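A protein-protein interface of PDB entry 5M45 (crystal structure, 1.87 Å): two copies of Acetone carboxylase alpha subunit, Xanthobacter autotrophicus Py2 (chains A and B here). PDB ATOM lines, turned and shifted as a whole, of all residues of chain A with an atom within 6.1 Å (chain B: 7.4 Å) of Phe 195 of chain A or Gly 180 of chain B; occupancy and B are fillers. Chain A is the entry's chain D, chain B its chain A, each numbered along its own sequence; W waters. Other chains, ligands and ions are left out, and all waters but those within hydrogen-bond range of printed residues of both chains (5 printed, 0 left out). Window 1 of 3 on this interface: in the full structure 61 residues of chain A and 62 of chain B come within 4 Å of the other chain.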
ATOM      1  N   VAL A 182     -12.719  -5.904  -7.750  1.00  0.00           N
ATOM      2  CA  VAL A 182     -12.520  -7.044  -6.836  1.00  0.00           C
ATOM      3  C   VAL A 182     -13.312  -8.287  -7.302  1.00  0.00           C
ATOM      4  O   VAL A 182     -12.750  -9.381  -7.393  1.00  0.00           O
ATOM      5  CB  VAL A 182     -12.889  -6.663  -5.366  1.00  0.00           C
ATOM      6  CG1 VAL A 182     -12.920  -7.877  -4.446  1.00  0.00           C
ATOM      7  CG2 VAL A 182     -11.906  -5.589  -4.852  1.00  0.00           C
ATOM      8  N   GLN A 191     -16.114  -5.612  -3.430  1.00  0.00           N
ATOM      9  CA  GLN A 191     -15.746  -4.267  -2.948  1.00  0.00           C
ATOM     10  C   GLN A 191     -16.973  -3.584  -2.317  1.00  0.00           C
ATOM     11  O   GLN A 191     -18.120  -3.906  -2.690  1.00  0.00           O
ATOM     12  CB  GLN A 191     -15.181  -3.405  -4.106  1.00  0.00           C
ATOM     13  CG  GLN A 191     -16.200  -2.956  -5.172  1.00  0.00           C
ATOM     14  CD  GLN A 191     -16.438  -3.954  -6.320  1.00  0.00           C
ATOM     15  OE1 GLN A 191     -16.109  -5.161  -6.263  1.00  0.00           O
ATOM     16  NE2 GLN A 191     -17.034  -3.453  -7.371  1.00  0.00           N
ATOM     17  N   VAL A 192     -16.739  -2.632  -1.413  1.00  0.00           N
ATOM     18  CA  VAL A 192     -17.791  -1.784  -0.815  1.00  0.00           C
ATOM     19  C   VAL A 192     -17.587  -0.269  -0.955  1.00  0.00           C
ATOM     20  O   VAL A 192     -18.414   0.517  -0.441  1.00  0.00           O
ATOM     21  CB  VAL A 192     -18.032  -2.126   0.672  1.00  0.00           C
ATOM     22  CG1 VAL A 192     -18.484  -3.569   0.792  1.00  0.00           C
ATOM     23  CG2 VAL A 192     -16.805  -1.886   1.542  1.00  0.00           C
ATOM     24  N   GLN A 193     -16.523   0.107  -1.692  1.00  0.00           N
ATOM     25  CA  GLN A 193     -16.081   1.467  -1.918  1.00  0.00           C
ATOM     26  C   GLN A 193     -15.471   1.612  -3.320  1.00  0.00           C
ATOM     27  O   GLN A 193     -15.198   0.635  -3.966  1.00  0.00           O
ATOM     28  CB  GLN A 193     -14.963   1.829  -0.938  1.00  0.00           C
ATOM     29  CG  GLN A 193     -15.340   1.899   0.510  1.00  0.00           C
ATOM     30  CD  GLN A 193     -14.124   2.290   1.357  1.00  0.00           C
ATOM     31  OE1 GLN A 193     -13.413   1.402   1.860  1.00  0.00           O
ATOM     32  NE2 GLN A 193     -13.901   3.561   1.560  1.00  0.00           N
ATOM     33  N   ARG A 194     -15.188   2.846  -3.726  1.00  0.00           N
ATOM     34  CA  ARG A 194     -14.481   3.189  -4.985  1.00  0.00           C
ATOM     35  C   ARG A 194     -13.161   2.416  -5.124  1.00  0.00           C
ATOM     36  O   ARG A 194     -12.778   2.047  -6.233  1.00  0.00           O
ATOM     37  CB  ARG A 194     -14.170   4.685  -4.988  1.00  0.00           C
ATOM     38  CG  ARG A 194     -13.485   5.278  -6.239  1.00  0.00           C
ATOM     39  CD  ARG A 194     -13.253   6.767  -6.113  1.00  0.00           C
ATOM     40  NE  ARG A 194     -12.892   7.370  -7.388  1.00  0.00           N
ATOM     41  CZ  ARG A 194     -13.690   7.531  -8.457  1.00  0.00           C
ATOM     42  NH1 ARG A 194     -14.966   7.215  -8.414  1.00  0.00           N
ATOM     43  NH2 ARG A 194     -13.210   8.081  -9.579  1.00  0.00           N
ATOM     44  N   PHE A 195     -12.504   2.213  -3.982  1.00  0.00           N
ATOM     45  CA  PHE A 195     -11.254   1.474  -3.885  1.00  0.00           C
ATOM     46  C   PHE A 195     -11.535  -0.037  -4.089  1.00  0.00           C
ATOM     47  O   PHE A 195     -12.022  -0.720  -3.193  1.00  0.00           O
ATOM     48  CB  PHE A 195     -10.573   1.821  -2.542  1.00  0.00           C
ATOM     49  CG  PHE A 195     -10.580   3.307  -2.235  1.00  0.00           C
ATOM     50  CD1 PHE A 195     -10.049   4.221  -3.142  1.00  0.00           C
ATOM     51  CD2 PHE A 195     -11.172   3.796  -1.077  1.00  0.00           C
ATOM     52  CE1 PHE A 195     -10.111   5.595  -2.899  1.00  0.00           C
ATOM     53  CE2 PHE A 195     -11.240   5.175  -0.835  1.00  0.00           C
ATOM     54  CZ  PHE A 195     -10.708   6.070  -1.763  1.00  0.00           C
ATOM     55  N   GLY A 196     -11.272  -0.544  -5.302  1.00  0.00           N
ATOM     56  CA  GLY A 196     -11.669  -1.893  -5.717  1.00  0.00           C
ATOM     57  C   GLY A 196     -12.898  -1.976  -6.640  1.00  0.00           C
ATOM     58  O   GLY A 196     -13.312  -3.084  -6.989  1.00  0.00           O
ATOM     59  N   ASP A 197     -13.477  -0.824  -7.037  1.00  0.00           N
ATOM     60  CA  ASP A 197     -14.696  -0.772  -7.844  1.00  0.00           C
ATOM     61  C   ASP A 197     -14.387  -0.778  -9.358  1.00  0.00           C
ATOM     62  O   ASP A 197     -15.308  -0.705 -10.175  1.00  0.00           O
ATOM     63  CB  ASP A 197     -15.525   0.475  -7.463  1.00  0.00           C
ATOM     64  CG  ASP A 197     -16.956   0.465  -7.996  1.00  0.00           C
ATOM     65  OD1 ASP A 197     -17.667  -0.581  -7.920  1.00  0.00           O
ATOM     66  OD2 ASP A 197     -17.411   1.575  -8.476  1.00  0.00           O
ATOM     67  N   GLY A 198     -13.099  -0.875  -9.730  1.00  0.00           N
ATOM     68  CA  GLY A 198     -12.681  -0.931 -11.118  1.00  0.00           C
ATOM     69  C   GLY A 198     -11.797   0.248 -11.554  1.00  0.00           C
ATOM     70  O   GLY A 198     -11.727   1.281 -10.884  1.00  0.00           O
ATOM     71  N   ARG A 393     -17.244  10.938  -1.668  1.00  0.00           N
ATOM     72  CA  ARG A 393     -16.408  10.558  -2.804  1.00  0.00           C
ATOM     73  C   ARG A 393     -15.910   9.115  -2.758  1.00  0.00           C
ATOM     74  O   ARG A 393     -15.228   8.714  -3.678  1.00  0.00           O
ATOM     75  CB  ARG A 393     -15.236  11.540  -2.983  1.00  0.00           C
ATOM     76  CG  ARG A 393     -14.165  11.482  -1.868  1.00  0.00           C
ATOM     77  CD  ARG A 393     -13.142  12.581  -2.086  1.00  0.00           C
ATOM     78  NE  ARG A 393     -12.107  12.624  -1.068  1.00  0.00           N
ATOM     79  CZ  ARG A 393     -10.971  11.910  -1.094  1.00  0.00           C
ATOM     80  NH1 ARG A 393     -10.673  11.078  -2.096  1.00  0.00           N
ATOM     81  NH2 ARG A 393     -10.084  12.085  -0.134  1.00  0.00           N
ATOM     82  N   ARG A 394     -16.249   8.355  -1.705  1.00  0.00           N
ATOM     83  CA  ARG A 394     -15.856   6.935  -1.592  1.00  0.00           C
ATOM     84  C   ARG A 394     -16.843   5.912  -2.107  1.00  0.00           C
ATOM     85  O   ARG A 394     -16.519   4.737  -2.098  1.00  0.00           O
ATOM     86  CB  ARG A 394     -15.498   6.579  -0.120  1.00  0.00           C
ATOM     87  CG  ARG A 394     -14.311   7.362   0.423  1.00  0.00           C
ATOM     88  CD  ARG A 394     -14.156   7.231   1.928  1.00  0.00           C
ATOM     89  NE  ARG A 394     -15.294   7.810   2.597  1.00  0.00           N
ATOM     90  CZ  ARG A 394     -15.637   7.610   3.869  1.00  0.00           C
ATOM     91  NH1 ARG A 394     -14.878   6.857   4.669  1.00  0.00           N
ATOM     92  NH2 ARG A 394     -16.725   8.200   4.349  1.00  0.00           N
ATOM     93  N   CYS B 152       2.529   2.044  -3.300  1.00  0.00           N
ATOM     94  CA  CYS B 152       2.800   3.233  -2.509  1.00  0.00           C
ATOM     95  C   CYS B 152       4.166   3.941  -2.726  1.00  0.00           C
ATOM     96  O   CYS B 152       4.360   5.073  -2.239  1.00  0.00           O
ATOM     97  CB  CYS B 152       2.558   2.986  -1.027  1.00  0.00           C
ATOM     98  SG  CYS B 152       0.789   2.986  -0.616  1.00  0.00           S
ATOM     99  N   ILE B 177       1.255   7.757   1.673  1.00  0.00           N
ATOM    100  CA  ILE B 177       0.481   7.130   2.745  1.00  0.00           C
ATOM    101  C   ILE B 177      -0.451   6.023   2.207  1.00  0.00           C
ATOM    102  O   ILE B 177      -0.515   4.923   2.790  1.00  0.00           O
ATOM    103  CB  ILE B 177      -0.311   8.159   3.601  1.00  0.00           C
ATOM    104  CG1 ILE B 177       0.651   9.157   4.250  1.00  0.00           C
ATOM    105  CG2 ILE B 177      -1.179   7.428   4.669  1.00  0.00           C
ATOM    106  CD1 ILE B 177      -0.040  10.372   4.866  1.00  0.00           C
ATOM    107  N   ASP B 178      -1.174   6.297   1.124  1.00  0.00           N
ATOM    108  CA  ASP B 178      -2.038   5.305   0.515  1.00  0.00           C
ATOM    109  C   ASP B 178      -2.239   5.550  -0.973  1.00  0.00           C
ATOM    110  O   ASP B 178      -2.089   6.704  -1.449  1.00  0.00           O
ATOM    111  CB  ASP B 178      -3.396   5.158   1.234  1.00  0.00           C
ATOM    112  CG  ASP B 178      -4.474   6.152   0.744  1.00  0.00           C
ATOM    113  OD1 ASP B 178      -4.424   7.354   1.104  1.00  0.00           O
ATOM    114  OD2 ASP B 178      -5.410   5.736   0.016  1.00  0.00           O
ATOM    115  N   THR B 179      -2.601   4.457  -1.687  1.00  0.00           N
ATOM    116  CA  THR B 179      -2.931   4.506  -3.090  1.00  0.00           C
ATOM    117  C   THR B 179      -4.339   3.979  -3.392  1.00  0.00           C
ATOM    118  O   THR B 179      -4.620   3.595  -4.520  1.00  0.00           O
ATOM    119  CB  THR B 179      -1.871   3.782  -3.977  1.00  0.00           C
ATOM    120  OG1 THR B 179      -1.529   2.510  -3.436  1.00  0.00           O
ATOM    121  CG2 THR B 179      -0.599   4.622  -4.054  1.00  0.00           C
ATOM    122  N   GLY B 180      -5.245   4.018  -2.423  1.00  0.00           N
ATOM    123  CA  GLY B 180      -6.624   3.629  -2.697  1.00  0.00           C
ATOM    124  C   GLY B 180      -6.766   2.140  -2.978  1.00  0.00           C
ATOM    125  O   GLY B 180      -7.465   1.745  -3.932  1.00  0.00           O
ATOM    126  N   ALA B 181      -6.118   1.323  -2.155  1.00  0.00           N
ATOM    127  CA  ALA B 181      -6.379  -0.135  -2.128  1.00  0.00           C
ATOM    128  C   ALA B 181      -7.605  -0.400  -1.270  1.00  0.00           C
ATOM    129  O   ALA B 181      -8.081   0.489  -0.555  1.00  0.00           O
ATOM    130  CB  ALA B 181      -5.162  -0.888  -1.590  1.00  0.00           C
ATOM    131  N   VAL B 182      -8.120  -1.626  -1.361  1.00  0.00           N
ATOM    132  CA  VAL B 182      -9.260  -2.103  -0.542  1.00  0.00           C
ATOM    133  C   VAL B 182      -9.021  -1.809   0.966  1.00  0.00           C
ATOM    134  O   VAL B 182      -9.897  -1.241   1.638  1.00  0.00           O
ATOM    135  CB  VAL B 182      -9.533  -3.603  -0.783  1.00  0.00           C
ATOM    136  CG1 VAL B 182     -10.535  -4.177   0.232  1.00  0.00           C
ATOM    137  CG2 VAL B 182     -10.017  -3.816  -2.232  1.00  0.00           C
ATOM    138  N   GLY B 183      -7.847  -2.164   1.461  1.00  0.00           N
ATOM    139  CA  GLY B 183      -7.458  -1.840   2.844  1.00  0.00           C
ATOM    140  C   GLY B 183      -6.865  -0.431   2.985  1.00  0.00           C
ATOM    141  O   GLY B 183      -6.081  -0.009   2.134  1.00  0.00           O
ATOM    142  N   PRO B 184      -7.214   0.285   4.074  1.00  0.00           N
ATOM    143  CA  PRO B 184      -6.725   1.639   4.317  1.00  0.00           C
ATOM    144  C   PRO B 184      -5.379   1.699   5.014  1.00  0.00           C
ATOM    145  O   PRO B 184      -5.297   1.651   6.239  1.00  0.00           O
ATOM    146  CB  PRO B 184      -7.804   2.240   5.220  1.00  0.00           C
ATOM    147  CG  PRO B 184      -8.329   1.073   6.002  1.00  0.00           C
ATOM    148  CD  PRO B 184      -8.267  -0.089   5.039  1.00  0.00           C
ATOM    149  N   GLY B 185      -4.331   1.831   4.224  1.00  0.00           N
ATOM    150  CA  GLY B 185      -2.942   1.876   4.687  1.00  0.00           C
ATOM    151  C   GLY B 185      -2.005   1.696   3.496  1.00  0.00           C
ATOM    152  O   GLY B 185      -2.476   1.487   2.360  1.00  0.00           O
ATOM    153  N   GLN B 191      -7.640  -6.959  -0.217  1.00  0.00           N
ATOM    154  CA  GLN B 191      -7.521  -7.475  -1.594  1.00  0.00           C
ATOM    155  C   GLN B 191      -6.598  -8.724  -1.614  1.00  0.00           C
ATOM    156  O   GLN B 191      -5.736  -8.873  -0.735  1.00  0.00           O
ATOM    157  CB  GLN B 191      -6.962  -6.388  -2.543  1.00  0.00           C
ATOM    158  CG  GLN B 191      -5.488  -6.017  -2.336  1.00  0.00           C
ATOM    159  CD  GLN B 191      -5.203  -4.943  -1.284  1.00  0.00           C
ATOM    160  OE1 GLN B 191      -6.028  -4.610  -0.426  1.00  0.00           O
ATOM    161  NE2 GLN B 191      -4.006  -4.407  -1.348  1.00  0.00           N
ATOM    162  N   PHE B 195      -6.391  -6.413  -8.737  1.00  0.00           N
ATOM    163  CA  PHE B 195      -7.715  -5.762  -8.748  1.00  0.00           C
ATOM    164  C   PHE B 195      -8.115  -5.406  -7.288  1.00  0.00           C
ATOM    165  O   PHE B 195      -8.514  -6.288  -6.502  1.00  0.00           O
ATOM    166  CB  PHE B 195      -8.710  -6.659  -9.477  1.00  0.00           C
ATOM    167  CG  PHE B 195      -8.157  -7.270 -10.744  1.00  0.00           C
ATOM    168  CD1 PHE B 195      -7.655  -6.452 -11.767  1.00  0.00           C
ATOM    169  CD2 PHE B 195      -8.114  -8.645 -10.920  1.00  0.00           C
ATOM    170  CE1 PHE B 195      -7.106  -7.010 -12.916  1.00  0.00           C
ATOM    171  CE2 PHE B 195      -7.575  -9.192 -12.106  1.00  0.00           C
ATOM    172  CZ  PHE B 195      -7.041  -8.373 -13.074  1.00  0.00           C
ATOM    173  N   GLY B 196      -7.940  -4.132  -6.915  1.00  0.00           N
ATOM    174  CA  GLY B 196      -8.061  -3.693  -5.504  1.00  0.00           C
ATOM    175  C   GLY B 196      -6.741  -3.444  -4.758  1.00  0.00           C
ATOM    176  O   GLY B 196      -6.769  -3.109  -3.569  1.00  0.00           O
ATOM    177  N   ASP B 197      -5.592  -3.598  -5.437  1.00  0.00           N
ATOM    178  CA  ASP B 197      -4.267  -3.477  -4.816  1.00  0.00           C
ATOM    179  C   ASP B 197      -3.745  -2.012  -4.865  1.00  0.00           C
ATOM    180  O   ASP B 197      -2.631  -1.745  -4.420  1.00  0.00           O
ATOM    181  CB  ASP B 197      -3.270  -4.425  -5.513  1.00  0.00           C
ATOM    182  CG  ASP B 197      -1.952  -4.618  -4.747  1.00  0.00           C
ATOM    183  OD1 ASP B 197      -1.952  -4.800  -3.474  1.00  0.00           O
ATOM    184  OD2 ASP B 197      -0.891  -4.648  -5.427  1.00  0.00           O
ATOM    185  N   GLY B 198      -4.550  -1.084  -5.392  1.00  0.00           N
ATOM    186  CA  GLY B 198      -4.155   0.325  -5.457  1.00  0.00           C
ATOM    187  C   GLY B 198      -4.063   0.880  -6.888  1.00  0.00           C
ATOM    188  O   GLY B 198      -3.973   0.135  -7.864  1.00  0.00           O
ATOM    189  N   TYR B 199      -4.099   2.193  -6.980  1.00  0.00           N
ATOM    190  CA  TYR B 199      -3.887   2.963  -8.234  1.00  0.00           C
ATOM    191  C   TYR B 199      -2.483   2.631  -8.795  1.00  0.00           C
ATOM    192  O   TYR B 199      -1.481   2.872  -8.126  1.00  0.00           O
ATOM    193  CB  TYR B 199      -3.983   4.457  -7.910  1.00  0.00           C
ATOM    194  CG  TYR B 199      -4.048   5.433  -9.098  1.00  0.00           C
ATOM    195  CD1 TYR B 199      -5.085   5.372 -10.029  1.00  0.00           C
ATOM    196  CD2 TYR B 199      -3.120   6.456  -9.226  1.00  0.00           C
ATOM    197  CE1 TYR B 199      -5.162   6.302 -11.095  1.00  0.00           C
ATOM    198  CE2 TYR B 199      -3.192   7.398 -10.256  1.00  0.00           C
ATOM    199  CZ  TYR B 199      -4.213   7.316 -11.197  1.00  0.00           C
ATOM    200  OH  TYR B 199      -4.299   8.278 -12.225  1.00  0.00           O
ATOM    201  N   GLN B 221      -5.889  12.377  -7.928  1.00  0.00           N
ATOM    202  CA  GLN B 221      -6.259  12.917  -6.624  1.00  0.00           C
ATOM    203  C   GLN B 221      -7.521  12.298  -6.025  1.00  0.00           C
ATOM    204  O   GLN B 221      -7.655  12.285  -4.794  1.00  0.00           O
ATOM    205  CB  GLN B 221      -6.359  14.452  -6.703  1.00  0.00           C
ATOM    206  CG  GLN B 221      -4.930  15.043  -6.813  1.00  0.00           C
ATOM    207  CD  GLN B 221      -4.862  16.485  -7.308  1.00  0.00           C
ATOM    208  OE1 GLN B 221      -5.848  17.233  -7.314  1.00  0.00           O
ATOM    209  NE2 GLN B 221      -3.686  16.876  -7.763  1.00  0.00           N
ATOM    210  N   ARG B 222      -8.432  11.800  -6.861  1.00  0.00           N
ATOM    211  CA  ARG B 222      -9.675  11.144  -6.413  1.00  0.00           C
ATOM    212  C   ARG B 222      -9.569   9.597  -6.310  1.00  0.00           C
ATOM    213  O   ARG B 222     -10.532   8.940  -5.876  1.00  0.00           O
ATOM    214  CB  ARG B 222     -10.855  11.518  -7.302  1.00  0.00           C
ATOM    215  CG  ARG B 222     -10.837  10.898  -8.704  1.00  0.00           C
ATOM    216  CD  ARG B 222     -11.907  11.510  -9.634  1.00  0.00           C
ATOM    217  NE  ARG B 222     -11.737  12.948  -9.745  1.00  0.00           N
ATOM    218  CZ  ARG B 222     -12.664  13.835 -10.115  1.00  0.00           C
ATOM    219  NH1 ARG B 222     -12.355  15.141 -10.068  1.00  0.00           N
ATOM    220  NH2 ARG B 222     -13.853  13.461 -10.585  1.00  0.00           N
ATOM    221  N   MET B 223      -8.416   9.027  -6.657  1.00  0.00           N
ATOM    222  CA  MET B 223      -8.210   7.592  -6.527  1.00  0.00           C
ATOM    223  C   MET B 223      -7.449   7.195  -5.235  1.00  0.00           C
ATOM    224  O   MET B 223      -7.062   6.010  -5.089  1.00  0.00           O
ATOM    225  CB  MET B 223      -7.462   7.050  -7.773  1.00  0.00           C
ATOM    226  CG  MET B 223      -8.222   7.150  -9.098  1.00  0.00           C
ATOM    227  SD  MET B 223      -9.952   6.673  -9.058  1.00  0.00           S
ATOM    228  CE  MET B 223      -9.834   4.910  -8.660  1.00  0.00           C
ATOM    229  N   VAL B 224      -7.250   8.148  -4.330  1.00  0.00           N
ATOM    230  CA  VAL B 224      -6.576   7.936  -3.036  1.00  0.00           C
ATOM    231  C   VAL B 224      -7.403   8.580  -1.901  1.00  0.00           C
ATOM    232  O   VAL B 224      -8.235   9.452  -2.130  1.00  0.00           O
ATOM    233  CB  VAL B 224      -5.104   8.471  -3.036  1.00  0.00           C
ATOM    234  CG1 VAL B 224      -4.313   7.933  -4.235  1.00  0.00           C
ATOM    235  CG2 VAL B 224      -5.011   9.995  -2.998  1.00  0.00           C
ATOM    236  N   ARG B 225      -7.191   8.083  -0.682  1.00  0.00           N
ATOM    237  CA  ARG B 225      -7.766   8.683   0.518  1.00  0.00           C
ATOM    238  C   ARG B 225      -7.075   9.988   0.936  1.00  0.00           C
ATOM    239  O   ARG B 225      -7.757  11.017   1.206  1.00  0.00           O
ATOM    240  CB  ARG B 225      -7.787   7.674   1.684  1.00  0.00           C
ATOM    241  CG  ARG B 225      -8.648   6.438   1.431  1.00  0.00           C
ATOM    242  CD  ARG B 225      -8.436   5.414   2.532  1.00  0.00           C
ATOM    243  NE  ARG B 225      -9.179   4.168   2.389  1.00  0.00           N
ATOM    244  CZ  ARG B 225      -8.849   3.143   1.600  1.00  0.00           C
ATOM    245  NH1 ARG B 225      -7.802   3.192   0.821  1.00  0.00           N
ATOM    246  NH2 ARG B 225      -9.600   2.025   1.601  1.00  0.00           N
ATOM    247  N   THR B 226      -5.739   9.954   1.004  1.00  0.00           N
ATOM    248  CA  THR B 226      -4.933  11.047   1.592  1.00  0.00           C
ATOM    249  C   THR B 226      -4.508  12.102   0.545  1.00  0.00           C
ATOM    250  O   THR B 226      -3.315  12.391   0.343  1.00  0.00           O
ATOM    251  CB  THR B 226      -3.721  10.470   2.373  1.00  0.00           C
ATOM    252  OG1 THR B 226      -2.970   9.570   1.533  1.00  0.00           O
ATOM    253  CG2 THR B 226      -4.234   9.734   3.645  1.00  0.00           C
ATOM    254  N   ILE B 450     -11.545  12.667   5.067  1.00  0.00           N
ATOM    255  CA  ILE B 450     -11.231  11.307   4.729  1.00  0.00           C
ATOM    256  C   ILE B 450      -9.720  11.122   4.873  1.00  0.00           C
ATOM    257  O   ILE B 450      -8.933  11.982   4.425  1.00  0.00           O
ATOM    258  CB  ILE B 450     -11.724  10.959   3.301  1.00  0.00           C
ATOM    259  CG1 ILE B 450     -13.273  10.952   3.272  1.00  0.00           C
ATOM    260  CG2 ILE B 450     -11.140   9.638   2.812  1.00  0.00           C
ATOM    261  CD1 ILE B 450     -13.877  10.813   1.889  1.00  0.00           C
HETATM  262  O   HOH W   1      -9.511  13.699   2.215  1.00  0.00           O
HETATM  263  O   HOH W   2     -11.286   8.275 -11.998  1.00  0.00           O
HETATM  264  O   HOH W   3     -12.463  10.080  -4.211  1.00  0.00           O
HETATM  265  O   HOH W   4     -11.915   4.347   3.496  1.00  0.00           O
HETATM  266  O   HOH W   5     -12.820  -1.477   1.447  1.00  0.00           O
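Of chain A, only Phe 195 (3.4 Å) comes within 4 Å of Gly 180 of chain B.
Of the printed residues of chain A, Arg 222 of chain B touches Arg 194 (3.2 Å).
Printed residues of chain B within 4 Å of Arg 194 of chain A: Arg 222 (3.2 Å) and Met 223 (3.5 Å).
Printed residues of chain B within 4 Å of Val 182 of chain A: Val 182 (3.7 Å) and Phe 195 (3.8 Å).
Of the printed residues of chain A, Val 224 of chain B touches Arg 393.
The nearest residue of chain A that does not touch Gly 180 of chain B is Gly 196 of chain A (4.6 Å).
The nearest printed residue of chain A that does not touch Ile 450 of chain B is Phe 195 of chain A (5.8 Å).
The backbone carbonyl oxygen of Val 182 of chain B is in hydrogen-bond range of the guanidinium group of Arg 225 of chain B.
OD2 of Asp 178 of chain B is in salt-bridge range of NH1 of Arg 225 of chain B, at 3.6 Å.
N of Gly 180 of chain B lies within hydrogen-bond range of OD2 of Asp 178 of chain B (3.0 Å).
The backbone NH (N) of Val 182 of chain A lies within hydrogen-bond range of the backbone carbonyl oxygen (O) of Gly 196 of chain A (3.0 Å).
The backbone carbonyl oxygen (O) of Ala 181 of chain B sits at hydrogen-bond distance from the guanidinium group (NH1) of Arg 225 of chain B (3.0 Å).
O of Arg 394 of chain A is in hydrogen-bond range of N of Arg 194 of chain A.
Printed residues of chain B that touch a printed residue of chain A: Gly 180, Ala 181, Val 182, Phe 195, Arg 222, Met 223, Val 224, Arg 225 and Ile 450.
Hydrophobic or aromatic side chains of chain B that line the printed part of chain A: Val 182, Met 223 and Ile 450.
Printed residues of chain A that touch a printed residue of chain B: Val 182, Gln 193, Arg 194, Phe 195, Arg 393 and Arg 394.
Hydrophobic or aromatic side chains of chain A within 4 Å of the printed part of chain B: Val 182 and Phe 195.
Among the printed residues, 14 pairs touch across the chains.
Among the printed residues, no Asp or Glu carboxylate lies within 4 Å of a Lys or Arg side-chain nitrogen of the other chain.
Among the printed residues, pairs that only touch across the chains: Arg 394 of chain A with Ile 450 of chain B (3.4 Å), Phe 195 of chain A with Gly 180 of chain B (3.4 Å), Phe 195 of chain A with Ala 181 of chain B (3.5 Å), Phe 195 of chain A with Arg 225 of chain B (3.6 Å), Val 182 of chain A with Val 182 of chain B (3.7 Å), Phe 195 of chain A with Met 223 of chain B (3.8 Å), Phe 195 of chain A with Val 182 of chain B (3.8 Å), Arg 393 of chain A with Ile 450 of chain B (3.8 Å), Val 182 of chain A with Phe 195 of chain B (3.8 Å) and Gln 193 of chain A with Arg 225 of chain B (3.9 Å).
Water W3 bridges O of Arg 222 of chain B and NH1 of Arg 393 of chain A.
Water W1 lies within hydrogen-bond range of O of Ile 450 of chain B, NH2 of Arg 393 of chain A and O of Arg 225 of chain B.
Water W4 lies within hydrogen-bond range of the side-chain amide nitrogen of Gln 193 of chain A (2.9 Å) and the guanidinium group of Arg 225 of chain B (3.0 Å).
Water W5 lies within hydrogen-bond range of the backbone carbonyl oxygen (O) of Val 182 of chain B (2.9 Å) and the side-chain amide oxygen (OE1) of Gln 193 of chain A (3.0 Å).
Water W2 bridges the guanidinium group (NH2) of Arg 194 of chain A (3.1 Å) and the side-chain sulfur (SD) of Met 223 of chain B (3.6 Å).
Val 182 of chain B touches its own counterpart, Val 182 of chain A.
Val 182 of chain A touches Phe 195 of chain B, and with the chains exchanged Phe 195 of chain A touches Val 182 of chain B.
Positions printed for both chains: 182, 191, 195, 196, 197 and 198.
The backbone carbonyl oxygen (O) of Arg 222 of chain B is in hydrogen-bond range of the guanidinium group (NE) of Arg 194 of chain A, 3.2 Å away.
O of Arg 225 of chain B lies within hydrogen-bond range of NH2 of Arg 393 of chain A (2.9 Å).
The backbone carbonyl oxygen of Val 224 of chain B lies within hydrogen-bond range of the guanidinium group of Arg 393 of chain A, 2.9 Å away.
NE of Arg 194 of chain A is in hydrogen-bond range of SD of Met 223 of chain B.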
